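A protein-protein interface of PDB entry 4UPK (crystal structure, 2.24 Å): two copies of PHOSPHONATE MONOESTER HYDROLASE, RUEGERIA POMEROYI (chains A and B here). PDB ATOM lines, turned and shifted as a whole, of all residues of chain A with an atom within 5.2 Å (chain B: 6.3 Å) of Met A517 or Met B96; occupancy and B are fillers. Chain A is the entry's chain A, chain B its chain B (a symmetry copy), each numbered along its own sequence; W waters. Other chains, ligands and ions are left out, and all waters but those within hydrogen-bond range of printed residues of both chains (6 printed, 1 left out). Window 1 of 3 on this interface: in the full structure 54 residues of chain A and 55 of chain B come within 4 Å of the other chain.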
ATOM      1  N   ASN A  97      29.558 -15.205   9.010  1.00  0.00           N
ATOM      2  CA  ASN A  97      30.768 -15.284   9.802  1.00  0.00           C
ATOM      3  C   ASN A  97      31.153 -13.949  10.462  1.00  0.00           C
ATOM      4  O   ASN A  97      31.388 -13.920  11.687  1.00  0.00           O
ATOM      5  CB  ASN A  97      31.905 -15.882   8.969  1.00  0.00           C
ATOM      6  CG  ASN A  97      31.674 -17.349   8.695  1.00  0.00           C
ATOM      7  OD1 ASN A  97      31.030 -18.052   9.472  1.00  0.00           O
ATOM      8  ND2 ASN A  97      32.170 -17.846   7.586  1.00  0.00           N
ATOM      9  N   ASP A 411      36.974 -16.434   4.286  1.00  0.00           N
ATOM     10  CA  ASP A 411      36.153 -17.377   3.508  1.00  0.00           C
ATOM     11  C   ASP A 411      36.465 -17.316   2.012  1.00  0.00           C
ATOM     12  O   ASP A 411      36.282 -18.316   1.312  1.00  0.00           O
ATOM     13  CB  ASP A 411      34.658 -17.096   3.719  1.00  0.00           C
ATOM     14  CG  ASP A 411      34.155 -17.337   5.132  1.00  0.00           C
ATOM     15  OD1 ASP A 411      34.472 -18.402   5.704  1.00  0.00           O
ATOM     16  OD2 ASP A 411      33.407 -16.486   5.643  1.00  0.00           O
ATOM     17  N   ARG A 513      26.591 -23.446   3.970  1.00  0.00           N
ATOM     18  CA  ARG A 513      26.561 -22.906   5.338  1.00  0.00           C
ATOM     19  C   ARG A 513      27.447 -23.764   6.252  1.00  0.00           C
ATOM     20  O   ARG A 513      28.237 -23.221   7.034  1.00  0.00           O
ATOM     21  CB  ARG A 513      25.129 -22.912   5.900  1.00  0.00           C
ATOM     22  CG  ARG A 513      24.212 -21.900   5.277  1.00  0.00           C
ATOM     23  CD  ARG A 513      23.210 -21.340   6.282  1.00  0.00           C
ATOM     24  NE  ARG A 513      22.548 -20.190   5.690  1.00  0.00           N
ATOM     25  CZ  ARG A 513      22.768 -18.925   6.015  1.00  0.00           C
ATOM     26  NH1 ARG A 513      23.557 -18.623   7.037  1.00  0.00           N
ATOM     27  NH2 ARG A 513      22.148 -17.956   5.369  1.00  0.00           N
ATOM     28  N   MET A 514      27.299 -25.110   6.147  1.00  0.00           N
ATOM     29  CA  MET A 514      28.065 -26.100   6.939  1.00  0.00           C
ATOM     30  C   MET A 514      29.542 -26.121   6.567  1.00  0.00           C
ATOM     31  O   MET A 514      30.374 -26.342   7.443  1.00  0.00           O
ATOM     32  CB  MET A 514      27.461 -27.509   6.800  1.00  0.00           C
ATOM     33  CG  MET A 514      26.038 -27.619   7.305  1.00  0.00           C
ATOM     34  SD  MET A 514      25.320 -29.254   7.079  1.00  0.00           S
ATOM     35  CE  MET A 514      26.062 -30.151   8.453  1.00  0.00           C
ATOM     36  N   ARG A 515      29.879 -25.851   5.279  1.00  0.00           N
ATOM     37  CA  ARG A 515      31.272 -25.822   4.808  1.00  0.00           C
ATOM     38  C   ARG A 515      31.973 -24.494   5.063  1.00  0.00           C
ATOM     39  O   ARG A 515      33.204 -24.417   4.962  1.00  0.00           O
ATOM     40  CB  ARG A 515      31.367 -26.172   3.325  1.00  0.00           C
ATOM     41  CG  ARG A 515      31.176 -27.645   3.013  1.00  0.00           C
ATOM     42  CD  ARG A 515      30.883 -27.772   1.532  1.00  0.00           C
ATOM     43  NE  ARG A 515      30.663 -29.158   1.129  1.00  0.00           N
ATOM     44  CZ  ARG A 515      30.202 -29.531  -0.059  1.00  0.00           C
ATOM     45  NH1 ARG A 515      29.884 -28.619  -0.972  1.00  0.00           N
ATOM     46  NH2 ARG A 515      30.041 -30.817  -0.340  1.00  0.00           N
ATOM     47  N   ASN A 516      31.206 -23.450   5.373  1.00  0.00           N
ATOM     48  CA  ASN A 516      31.756 -22.121   5.613  1.00  0.00           C
ATOM     49  C   ASN A 516      31.329 -21.541   6.961  1.00  0.00           C
ATOM     50  O   ASN A 516      30.858 -20.402   7.018  1.00  0.00           O
ATOM     51  CB  ASN A 516      31.474 -21.153   4.429  1.00  0.00           C
ATOM     52  CG  ASN A 516      32.006 -21.637   3.105  1.00  0.00           C
ATOM     53  OD1 ASN A 516      33.163 -21.408   2.738  1.00  0.00           O
ATOM     54  ND2 ASN A 516      31.192 -22.404   2.403  1.00  0.00           N
ATOM     55  N   MET A 517      31.536 -22.312   8.054  1.00  0.00           N
ATOM     56  CA  MET A 517      31.297 -21.839   9.416  1.00  0.00           C
ATOM     57  C   MET A 517      32.560 -21.091   9.844  1.00  0.00           C
ATOM     58  O   MET A 517      33.560 -21.170   9.127  1.00  0.00           O
ATOM     59  CB  MET A 517      30.990 -22.990  10.372  1.00  0.00           C
ATOM     60  CG  MET A 517      29.559 -23.436  10.318  1.00  0.00           C
ATOM     61  SD  MET A 517      29.248 -24.711  11.551  1.00  0.00           S
ATOM     62  CE  MET A 517      29.718 -26.126  10.660  1.00  0.00           C
ATOM     63  N   ASP A 518      32.521 -20.350  10.975  1.00  0.00           N
ATOM     64  CA  ASP A 518      33.662 -19.551  11.447  1.00  0.00           C
ATOM     65  C   ASP A 518      34.985 -20.331  11.572  1.00  0.00           C
ATOM     66  O   ASP A 518      35.109 -21.192  12.443  1.00  0.00           O
ATOM     67  CB  ASP A 518      33.313 -18.804  12.750  1.00  0.00           C
ATOM     68  CG  ASP A 518      34.179 -17.584  13.033  1.00  0.00           C
ATOM     69  OD1 ASP A 518      35.360 -17.577  12.622  1.00  0.00           O
ATOM     70  OD2 ASP A 518      33.687 -16.651  13.685  1.00  0.00           O
ATOM     71  N   HIS A 519      35.971 -20.017  10.701  1.00  0.00           N
ATOM     72  CA  HIS A 519      37.292 -20.686  10.668  1.00  0.00           C
ATOM     73  C   HIS A 519      38.426 -19.983  11.458  1.00  0.00           C
ATOM     74  O   HIS A 519      39.589 -20.386  11.318  1.00  0.00           O
ATOM     75  CB  HIS A 519      37.743 -20.916   9.210  1.00  0.00           C
ATOM     76  CG  HIS A 519      37.155 -22.122   8.562  1.00  0.00           C
ATOM     77  ND1 HIS A 519      35.810 -22.192   8.251  1.00  0.00           N
ATOM     78  CD2 HIS A 519      37.763 -23.247   8.124  1.00  0.00           C
ATOM     79  CE1 HIS A 519      35.643 -23.350   7.642  1.00  0.00           C
ATOM     80  NE2 HIS A 519      36.782 -24.035   7.576  1.00  0.00           N
ATOM     81  N   ARG A 536      43.818 -23.217   5.675  1.00  0.00           N
ATOM     82  CA  ARG A 536      42.458 -23.436   5.158  1.00  0.00           C
ATOM     83  C   ARG A 536      42.424 -23.730   3.678  1.00  0.00           C
ATOM     84  O   ARG A 536      41.754 -24.675   3.234  1.00  0.00           O
ATOM     85  CB  ARG A 536      41.533 -22.246   5.493  1.00  0.00           C
ATOM     86  CG  ARG A 536      40.070 -22.522   5.201  1.00  0.00           C
ATOM     87  CD  ARG A 536      39.217 -21.291   5.414  1.00  0.00           C
ATOM     88  NE  ARG A 536      37.864 -21.464   4.871  1.00  0.00           N
ATOM     89  CZ  ARG A 536      36.834 -20.682   5.170  1.00  0.00           C
ATOM     90  NH1 ARG A 536      36.986 -19.671   6.017  1.00  0.00           N
ATOM     91  NH2 ARG A 536      35.637 -20.916   4.636  1.00  0.00           N
ATOM     92  N   GLN B  93      25.781 -22.327  24.035  1.00  0.00           N
ATOM     93  CA  GLN B  93      25.764 -22.136  22.574  1.00  0.00           C
ATOM     94  C   GLN B  93      25.910 -23.444  21.808  1.00  0.00           C
ATOM     95  O   GLN B  93      26.529 -24.379  22.288  1.00  0.00           O
ATOM     96  CB  GLN B  93      26.924 -21.237  22.130  1.00  0.00           C
ATOM     97  CG  GLN B  93      27.014 -19.873  22.798  1.00  0.00           C
ATOM     98  CD  GLN B  93      28.171 -19.064  22.255  1.00  0.00           C
ATOM     99  OE1 GLN B  93      28.728 -19.350  21.187  1.00  0.00           O
ATOM    100  NE2 GLN B  93      28.536 -18.002  22.959  1.00  0.00           N
ATOM    101  N   TYR B  94      25.412 -23.475  20.573  1.00  0.00           N
ATOM    102  CA  TYR B  94      25.573 -24.611  19.665  1.00  0.00           C
ATOM    103  C   TYR B  94      27.042 -24.648  19.209  1.00  0.00           C
ATOM    104  O   TYR B  94      27.705 -23.612  19.244  1.00  0.00           O
ATOM    105  CB  TYR B  94      24.648 -24.447  18.432  1.00  0.00           C
ATOM    106  CG  TYR B  94      23.167 -24.625  18.725  1.00  0.00           C
ATOM    107  CD1 TYR B  94      22.641 -25.876  19.054  1.00  0.00           C
ATOM    108  CD2 TYR B  94      22.279 -23.562  18.591  1.00  0.00           C
ATOM    109  CE1 TYR B  94      21.273 -26.052  19.272  1.00  0.00           C
ATOM    110  CE2 TYR B  94      20.922 -23.716  18.849  1.00  0.00           C
ATOM    111  CZ  TYR B  94      20.420 -24.964  19.174  1.00  0.00           C
ATOM    112  OH  TYR B  94      19.075 -25.088  19.426  1.00  0.00           O
ATOM    113  N   ALA B  95      27.548 -25.840  18.766  1.00  0.00           N
ATOM    114  CA  ALA B  95      28.911 -25.980  18.261  1.00  0.00           C
ATOM    115  C   ALA B  95      29.158 -25.067  17.065  1.00  0.00           C
ATOM    116  O   ALA B  95      30.276 -24.572  16.918  1.00  0.00           O
ATOM    117  CB  ALA B  95      29.210 -27.420  17.901  1.00  0.00           C
ATOM    118  N   MET B  96      28.111 -24.804  16.235  1.00  0.00           N
ATOM    119  CA  MET B  96      28.177 -23.874  15.091  1.00  0.00           C
ATOM    120  C   MET B  96      28.490 -22.429  15.531  1.00  0.00           C
ATOM    121  O   MET B  96      29.090 -21.683  14.772  1.00  0.00           O
ATOM    122  CB  MET B  96      26.941 -23.958  14.157  1.00  0.00           C
ATOM    123  CG  MET B  96      25.617 -23.641  14.815  1.00  0.00           C
ATOM    124  SD  MET B  96      24.202 -23.980  13.742  1.00  0.00           S
ATOM    125  CE  MET B  96      22.875 -23.569  14.859  1.00  0.00           C
ATOM    126  N   ASN B  97      28.151 -22.063  16.780  1.00  0.00           N
ATOM    127  CA  ASN B  97      28.487 -20.757  17.356  1.00  0.00           C
ATOM    128  C   ASN B  97      29.815 -20.750  18.116  1.00  0.00           C
ATOM    129  O   ASN B  97      30.704 -20.012  17.712  1.00  0.00           O
ATOM    130  CB  ASN B  97      27.314 -20.164  18.139  1.00  0.00           C
ATOM    131  CG  ASN B  97      26.187 -19.815  17.205  1.00  0.00           C
ATOM    132  OD1 ASN B  97      26.411 -19.385  16.079  1.00  0.00           O
ATOM    133  ND2 ASN B  97      24.965 -20.103  17.583  1.00  0.00           N
ATOM    134  N   HIS B  98      29.989 -21.613  19.158  1.00  0.00           N
ATOM    135  CA  HIS B  98      31.251 -21.684  19.924  1.00  0.00           C
ATOM    136  C   HIS B  98      32.469 -22.205  19.136  1.00  0.00           C
ATOM    137  O   HIS B  98      33.603 -21.885  19.484  1.00  0.00           O
ATOM    138  CB  HIS B  98      31.078 -22.351  21.301  1.00  0.00           C
ATOM    139  CG  HIS B  98      30.892 -23.832  21.278  1.00  0.00           C
ATOM    140  ND1 HIS B  98      31.814 -24.669  20.681  1.00  0.00           N
ATOM    141  CD2 HIS B  98      29.944 -24.583  21.868  1.00  0.00           C
ATOM    142  CE1 HIS B  98      31.362 -25.895  20.871  1.00  0.00           C
ATOM    143  NE2 HIS B  98      30.258 -25.893  21.611  1.00  0.00           N
ATOM    144  N   ARG B  99      32.222 -23.000  18.082  1.00  0.00           N
ATOM    145  CA  ARG B  99      33.213 -23.518  17.121  1.00  0.00           C
ATOM    146  C   ARG B  99      34.354 -24.444  17.645  1.00  0.00           C
ATOM    147  O   ARG B  99      35.206 -24.885  16.873  1.00  0.00           O
ATOM    148  CB  ARG B  99      33.655 -22.429  16.114  1.00  0.00           C
ATOM    149  CG  ARG B  99      32.536 -21.964  15.157  1.00  0.00           C
ATOM    150  CD  ARG B  99      32.139 -23.041  14.139  1.00  0.00           C
ATOM    151  NE  ARG B  99      33.216 -23.284  13.179  1.00  0.00           N
ATOM    152  CZ  ARG B  99      33.401 -24.427  12.535  1.00  0.00           C
ATOM    153  NH1 ARG B  99      32.584 -25.451  12.738  1.00  0.00           N
ATOM    154  NH2 ARG B  99      34.397 -24.552  11.672  1.00  0.00           N
ATOM    155  N   VAL B 101      34.670 -27.506  17.844  1.00  0.00           N
ATOM    156  CA  VAL B 101      33.970 -28.621  17.202  1.00  0.00           C
ATOM    157  C   VAL B 101      34.537 -30.020  17.423  1.00  0.00           C
ATOM    158  O   VAL B 101      33.812 -31.007  17.229  1.00  0.00           O
ATOM    159  CB  VAL B 101      33.554 -28.327  15.723  1.00  0.00           C
ATOM    160  CG1 VAL B 101      32.661 -27.092  15.640  1.00  0.00           C
ATOM    161  CG2 VAL B 101      34.763 -28.186  14.811  1.00  0.00           C
ATOM    162  N   ASP B 411      22.472 -19.480  23.008  1.00  0.00           N
ATOM    163  CA  ASP B 411      21.462 -20.055  22.117  1.00  0.00           C
ATOM    164  C   ASP B 411      20.349 -20.769  22.890  1.00  0.00           C
ATOM    165  O   ASP B 411      19.222 -20.838  22.395  1.00  0.00           O
ATOM    166  CB  ASP B 411      22.114 -21.050  21.132  1.00  0.00           C
ATOM    167  CG  ASP B 411      23.085 -20.430  20.152  1.00  0.00           C
ATOM    168  OD1 ASP B 411      22.735 -19.386  19.538  1.00  0.00           O
ATOM    169  OD2 ASP B 411      24.179 -20.999  19.970  1.00  0.00           O
ATOM    170  N   PHE B 432      18.235 -30.381  18.155  1.00  0.00           N
ATOM    171  CA  PHE B 432      19.308 -30.280  17.199  1.00  0.00           C
ATOM    172  C   PHE B 432      20.679 -30.643  17.792  1.00  0.00           C
ATOM    173  O   PHE B 432      21.059 -30.130  18.851  1.00  0.00           O
ATOM    174  CB  PHE B 432      19.304 -28.844  16.658  1.00  0.00           C
ATOM    175  CG  PHE B 432      20.344 -28.533  15.625  1.00  0.00           C
ATOM    176  CD1 PHE B 432      20.101 -28.781  14.273  1.00  0.00           C
ATOM    177  CD2 PHE B 432      21.547 -27.931  15.987  1.00  0.00           C
ATOM    178  CE1 PHE B 432      21.057 -28.446  13.305  1.00  0.00           C
ATOM    179  CE2 PHE B 432      22.493 -27.587  15.016  1.00  0.00           C
ATOM    180  CZ  PHE B 432      22.250 -27.857  13.688  1.00  0.00           C
ATOM    181  N   GLU B 434      25.043 -31.637  16.617  1.00  0.00           N
ATOM    182  CA  GLU B 434      26.115 -31.529  15.633  1.00  0.00           C
ATOM    183  C   GLU B 434      27.289 -32.445  15.967  1.00  0.00           C
ATOM    184  O   GLU B 434      27.510 -32.797  17.118  1.00  0.00           O
ATOM    185  CB  GLU B 434      26.619 -30.080  15.531  1.00  0.00           C
ATOM    186  CG  GLU B 434      25.635 -29.108  14.917  1.00  0.00           C
ATOM    187  CD  GLU B 434      26.202 -27.708  14.848  1.00  0.00           C
ATOM    188  OE1 GLU B 434      26.940 -27.415  13.880  1.00  0.00           O
ATOM    189  OE2 GLU B 434      25.995 -26.938  15.813  1.00  0.00           O
ATOM    190  N   ASP B 436      31.556 -33.360  14.249  1.00  0.00           N
ATOM    191  CA  ASP B 436      32.591 -33.070  13.257  1.00  0.00           C
ATOM    192  C   ASP B 436      33.376 -34.357  13.078  1.00  0.00           C
ATOM    193  O   ASP B 436      33.759 -34.962  14.064  1.00  0.00           O
ATOM    194  CB  ASP B 436      33.495 -31.880  13.635  1.00  0.00           C
ATOM    195  CG  ASP B 436      34.199 -31.278  12.429  1.00  0.00           C
ATOM    196  OD1 ASP B 436      35.029 -31.969  11.818  1.00  0.00           O
ATOM    197  OD2 ASP B 436      33.910 -30.133  12.095  1.00  0.00           O
ATOM    198  N   SER B 455      37.326 -28.655   6.528  1.00  0.00           N
ATOM    199  CA  SER B 455      36.310 -27.595   6.473  1.00  0.00           C
ATOM    200  C   SER B 455      34.925 -28.240   6.190  1.00  0.00           C
ATOM    201  O   SER B 455      33.899 -27.554   6.309  1.00  0.00           O
ATOM    202  CB  SER B 455      36.620 -26.581   5.364  1.00  0.00           C
ATOM    203  OG  SER B 455      37.703 -25.720   5.683  1.00  0.00           O
ATOM    204  N   ALA B 458      31.568 -31.352   9.234  1.00  0.00           N
ATOM    205  CA  ALA B 458      30.330 -31.150  10.004  1.00  0.00           C
ATOM    206  C   ALA B 458      29.126 -32.049   9.606  1.00  0.00           C
ATOM    207  O   ALA B 458      28.814 -32.265   8.421  1.00  0.00           O
ATOM    208  CB  ALA B 458      29.925 -29.693   9.983  1.00  0.00           C
ATOM    209  N   HIS B 512      16.934 -23.577  11.102  1.00  0.00           N
ATOM    210  CA  HIS B 512      17.517 -23.628  12.447  1.00  0.00           C
ATOM    211  C   HIS B 512      18.928 -23.009  12.468  1.00  0.00           C
ATOM    212  O   HIS B 512      19.236 -22.222  13.363  1.00  0.00           O
ATOM    213  CB  HIS B 512      17.540 -25.075  12.994  1.00  0.00           C
ATOM    214  CG  HIS B 512      18.137 -25.164  14.362  1.00  0.00           C
ATOM    215  ND1 HIS B 512      17.385 -24.915  15.485  1.00  0.00           N
ATOM    216  CD2 HIS B 512      19.416 -25.401  14.731  1.00  0.00           C
ATOM    217  CE1 HIS B 512      18.219 -25.003  16.498  1.00  0.00           C
ATOM    218  NE2 HIS B 512      19.450 -25.305  16.091  1.00  0.00           N
ATOM    219  N   ARG B 513      19.775 -23.378  11.496  1.00  0.00           N
ATOM    220  CA  ARG B 513      21.121 -22.836  11.360  1.00  0.00           C
ATOM    221  C   ARG B 513      21.059 -21.323  11.124  1.00  0.00           C
ATOM    222  O   ARG B 513      21.798 -20.592  11.779  1.00  0.00           O
ATOM    223  CB  ARG B 513      21.891 -23.504  10.208  1.00  0.00           C
ATOM    224  CG  ARG B 513      21.981 -25.019  10.270  1.00  0.00           C
ATOM    225  CD  ARG B 513      23.023 -25.480   9.273  1.00  0.00           C
ATOM    226  NE  ARG B 513      24.364 -25.310   9.832  1.00  0.00           N
ATOM    227  CZ  ARG B 513      25.023 -26.245  10.499  1.00  0.00           C
ATOM    228  NH1 ARG B 513      24.495 -27.453  10.660  1.00  0.00           N
ATOM    229  NH2 ARG B 513      26.222 -25.985  11.005  1.00  0.00           N
ATOM    230  N   MET B 514      20.175 -20.859  10.208  1.00  0.00           N
ATOM    231  CA  MET B 514      19.965 -19.429   9.896  1.00  0.00           C
ATOM    232  C   MET B 514      19.375 -18.649  11.094  1.00  0.00           C
ATOM    233  O   MET B 514      19.709 -17.480  11.271  1.00  0.00           O
ATOM    234  CB  MET B 514      19.040 -19.258   8.686  1.00  0.00           C
ATOM    235  CG  MET B 514      19.596 -19.825   7.385  1.00  0.00           C
ATOM    236  SD  MET B 514      18.446 -19.700   6.004  1.00  0.00           S
ATOM    237  CE  MET B 514      18.650 -17.975   5.545  1.00  0.00           C
ATOM    238  N   ASN B 516      19.906 -19.470  14.279  1.00  0.00           N
ATOM    239  CA  ASN B 516      20.846 -19.580  15.390  1.00  0.00           C
ATOM    240  C   ASN B 516      22.285 -19.320  14.987  1.00  0.00           C
ATOM    241  O   ASN B 516      23.151 -20.145  15.241  1.00  0.00           O
ATOM    242  CB  ASN B 516      20.686 -20.929  16.118  1.00  0.00           C
ATOM    243  CG  ASN B 516      19.316 -21.150  16.677  1.00  0.00           C
ATOM    244  OD1 ASN B 516      19.029 -20.780  17.806  1.00  0.00           O
ATOM    245  ND2 ASN B 516      18.429 -21.735  15.884  1.00  0.00           N
ATOM    246  N   MET B 517      22.548 -18.181  14.343  1.00  0.00           N
ATOM    247  CA  MET B 517      23.914 -17.741  13.993  1.00  0.00           C
ATOM    248  C   MET B 517      24.444 -16.970  15.212  1.00  0.00           C
ATOM    249  O   MET B 517      23.666 -16.677  16.114  1.00  0.00           O
ATOM    250  CB  MET B 517      23.920 -16.848  12.740  1.00  0.00           C
ATOM    251  CG  MET B 517      23.839 -17.631  11.459  1.00  0.00           C
ATOM    252  SD  MET B 517      23.958 -16.531  10.055  1.00  0.00           S
ATOM    253  CE  MET B 517      22.225 -16.023   9.853  1.00  0.00           C
ATOM    254  N   ASP B 518      25.749 -16.668  15.256  1.00  0.00           N
ATOM    255  CA  ASP B 518      26.375 -15.963  16.378  1.00  0.00           C
ATOM    256  C   ASP B 518      25.684 -14.629  16.781  1.00  0.00           C
ATOM    257  O   ASP B 518      25.756 -13.637  16.046  1.00  0.00           O
ATOM    258  CB  ASP B 518      27.878 -15.764  16.126  1.00  0.00           C
ATOM    259  CG  ASP B 518      28.713 -15.537  17.376  1.00  0.00           C
ATOM    260  OD1 ASP B 518      28.183 -14.977  18.352  1.00  0.00           O
ATOM    261  OD2 ASP B 518      29.885 -15.949  17.383  1.00  0.00           O
HETATM  262  O   HOH W   1      30.060 -20.260  12.834  1.00  0.00           O
HETATM  263  O   HOH W   2      20.445 -20.471   3.846  1.00  0.00           O
HETATM  264  O   HOH W   3      23.004 -28.586   8.702  1.00  0.00           O
HETATM  265  O   HOH W   4      31.905 -28.556   7.847  1.00  0.00           O
HETATM  266  O   HOH W   5      40.046 -26.653   5.211  1.00  0.00           O
HETATM  267  O   HOH W   6      29.578 -26.874  14.138  1.00  0.00           O
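The guanidinium group (NH1) of Arg A513 sits at hydrogen-bond distance from the side-chain sulfur (SD) of Met B517, 3.7 Å away. SD of Met A517 sits close to NH1 of Arg B99 (3.6 Å). The guanidinium group (NH2) of Arg B513 is in hydrogen-bond range of the side-chain sulfur (SD) of Met A517 (3.3 Å). NE of Arg B99 is in hydrogen-bond range of O of Asp A518 (2.9 Å). NE2 of His A519 lies within hydrogen-bond range of OG of Ser B455 (2.7 Å). The backbone carbonyl oxygen (O) of Ser B455 sits close to the backbone carbonyl oxygen (O) of Arg A515 (3.5 Å).
OD1 of Asn A97 sits at hydrogen-bond distance from N of Asp A518 (3.1 Å). O of Met A517 lies within hydrogen-bond range of ND1 of His A519 (2.6 Å). The backbone NH (N) of Met B96 is in hydrogen-bond range of the side-chain carboxylate (OE2) of Glu B434. OE1 of Glu B434 is in salt-bridge range of NH2 of Arg B513, 3.3 Å away.
Arg A513 touches Met B514. O of Ser B455 touches O of Met A514, 3.9 Å away. Met A514 touches Ala B458. Met A514 touches Arg B513. Met B96 touches Met A517 (CB to SD, 3.6 Å). CB of Ala B458 touches CE of Met A517, 3.6 Å away.
Asp A411 touches none of the printed residues of chain B. Of the printed residues of chain B, Arg A513 touches Met B514 (3.4 Å) and Met B517 (3.7 Å). Of the printed residues of chain B, Arg A515 touches Ser B455 (3.5 Å). Of chain A, only Met A517 (3.6 Å) comes within 4 Å of Met B96. Asn B97 touches none of the printed residues of chain A. Printed residues of chain A within 4 Å of Arg B99: Met A517 (3.5 Å) and Asp A518 (2.9 Å). Of the printed residues of chain A, Met B514 touches Arg A513. Of the printed residues of chain A, Met B517 touches Arg A513 (3.7 Å). The nearest residue of chain B that does not touch Met A517 is Glu B434 (4.3 Å).
Hydrophobic or aromatic side chains of chain B that line the printed part of chain A: Met B96, Ala B458, Met B514 and Met B517. Among the printed residues, no Asp or Glu carboxylate lies within 4 Å of a Lys or Arg side-chain nitrogen of the other chain.
Arg A513 touches Met B514, and with the chains exchanged Met A514 touches Arg B513. Arg A513 touches Met B517, and with the chains exchanged Met A517 touches Arg B513. Positions printed for both chains: 97, 411, 513, 514, 516, 517 and 518. Of the 12 pairs that touch across the chains among the printed residues, 4 have their exchanged pair printed and touching as well.
Water W5 bridges OG of Ser B455 (2.6 Å) and O of Arg A536 (3.3 Å). Water W1 lies within hydrogen-bond range of the backbone carbonyl oxygen of Met B96 (2.6 Å) and the backbone NH of Asp A518 (3.1 Å). Water W6 lies within hydrogen-bond range of OE1 of Glu B434, N of Met B96 and SD of Met A517. Water W3 bridges the guanidinium group of Arg B513 (2.7 Å) and the side-chain sulfur of Met A514 (2.9 Å). Water W4 lies within hydrogen-bond range of O of Ser B455 (2.7 Å), O of Met A514 (2.7 Å) and N of Ala B458 (3.1 Å). Water W2 bridges the guanidinium group of Arg A513 (2.8 Å) and the side-chain sulfur of Met B514 (3.0 Å).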
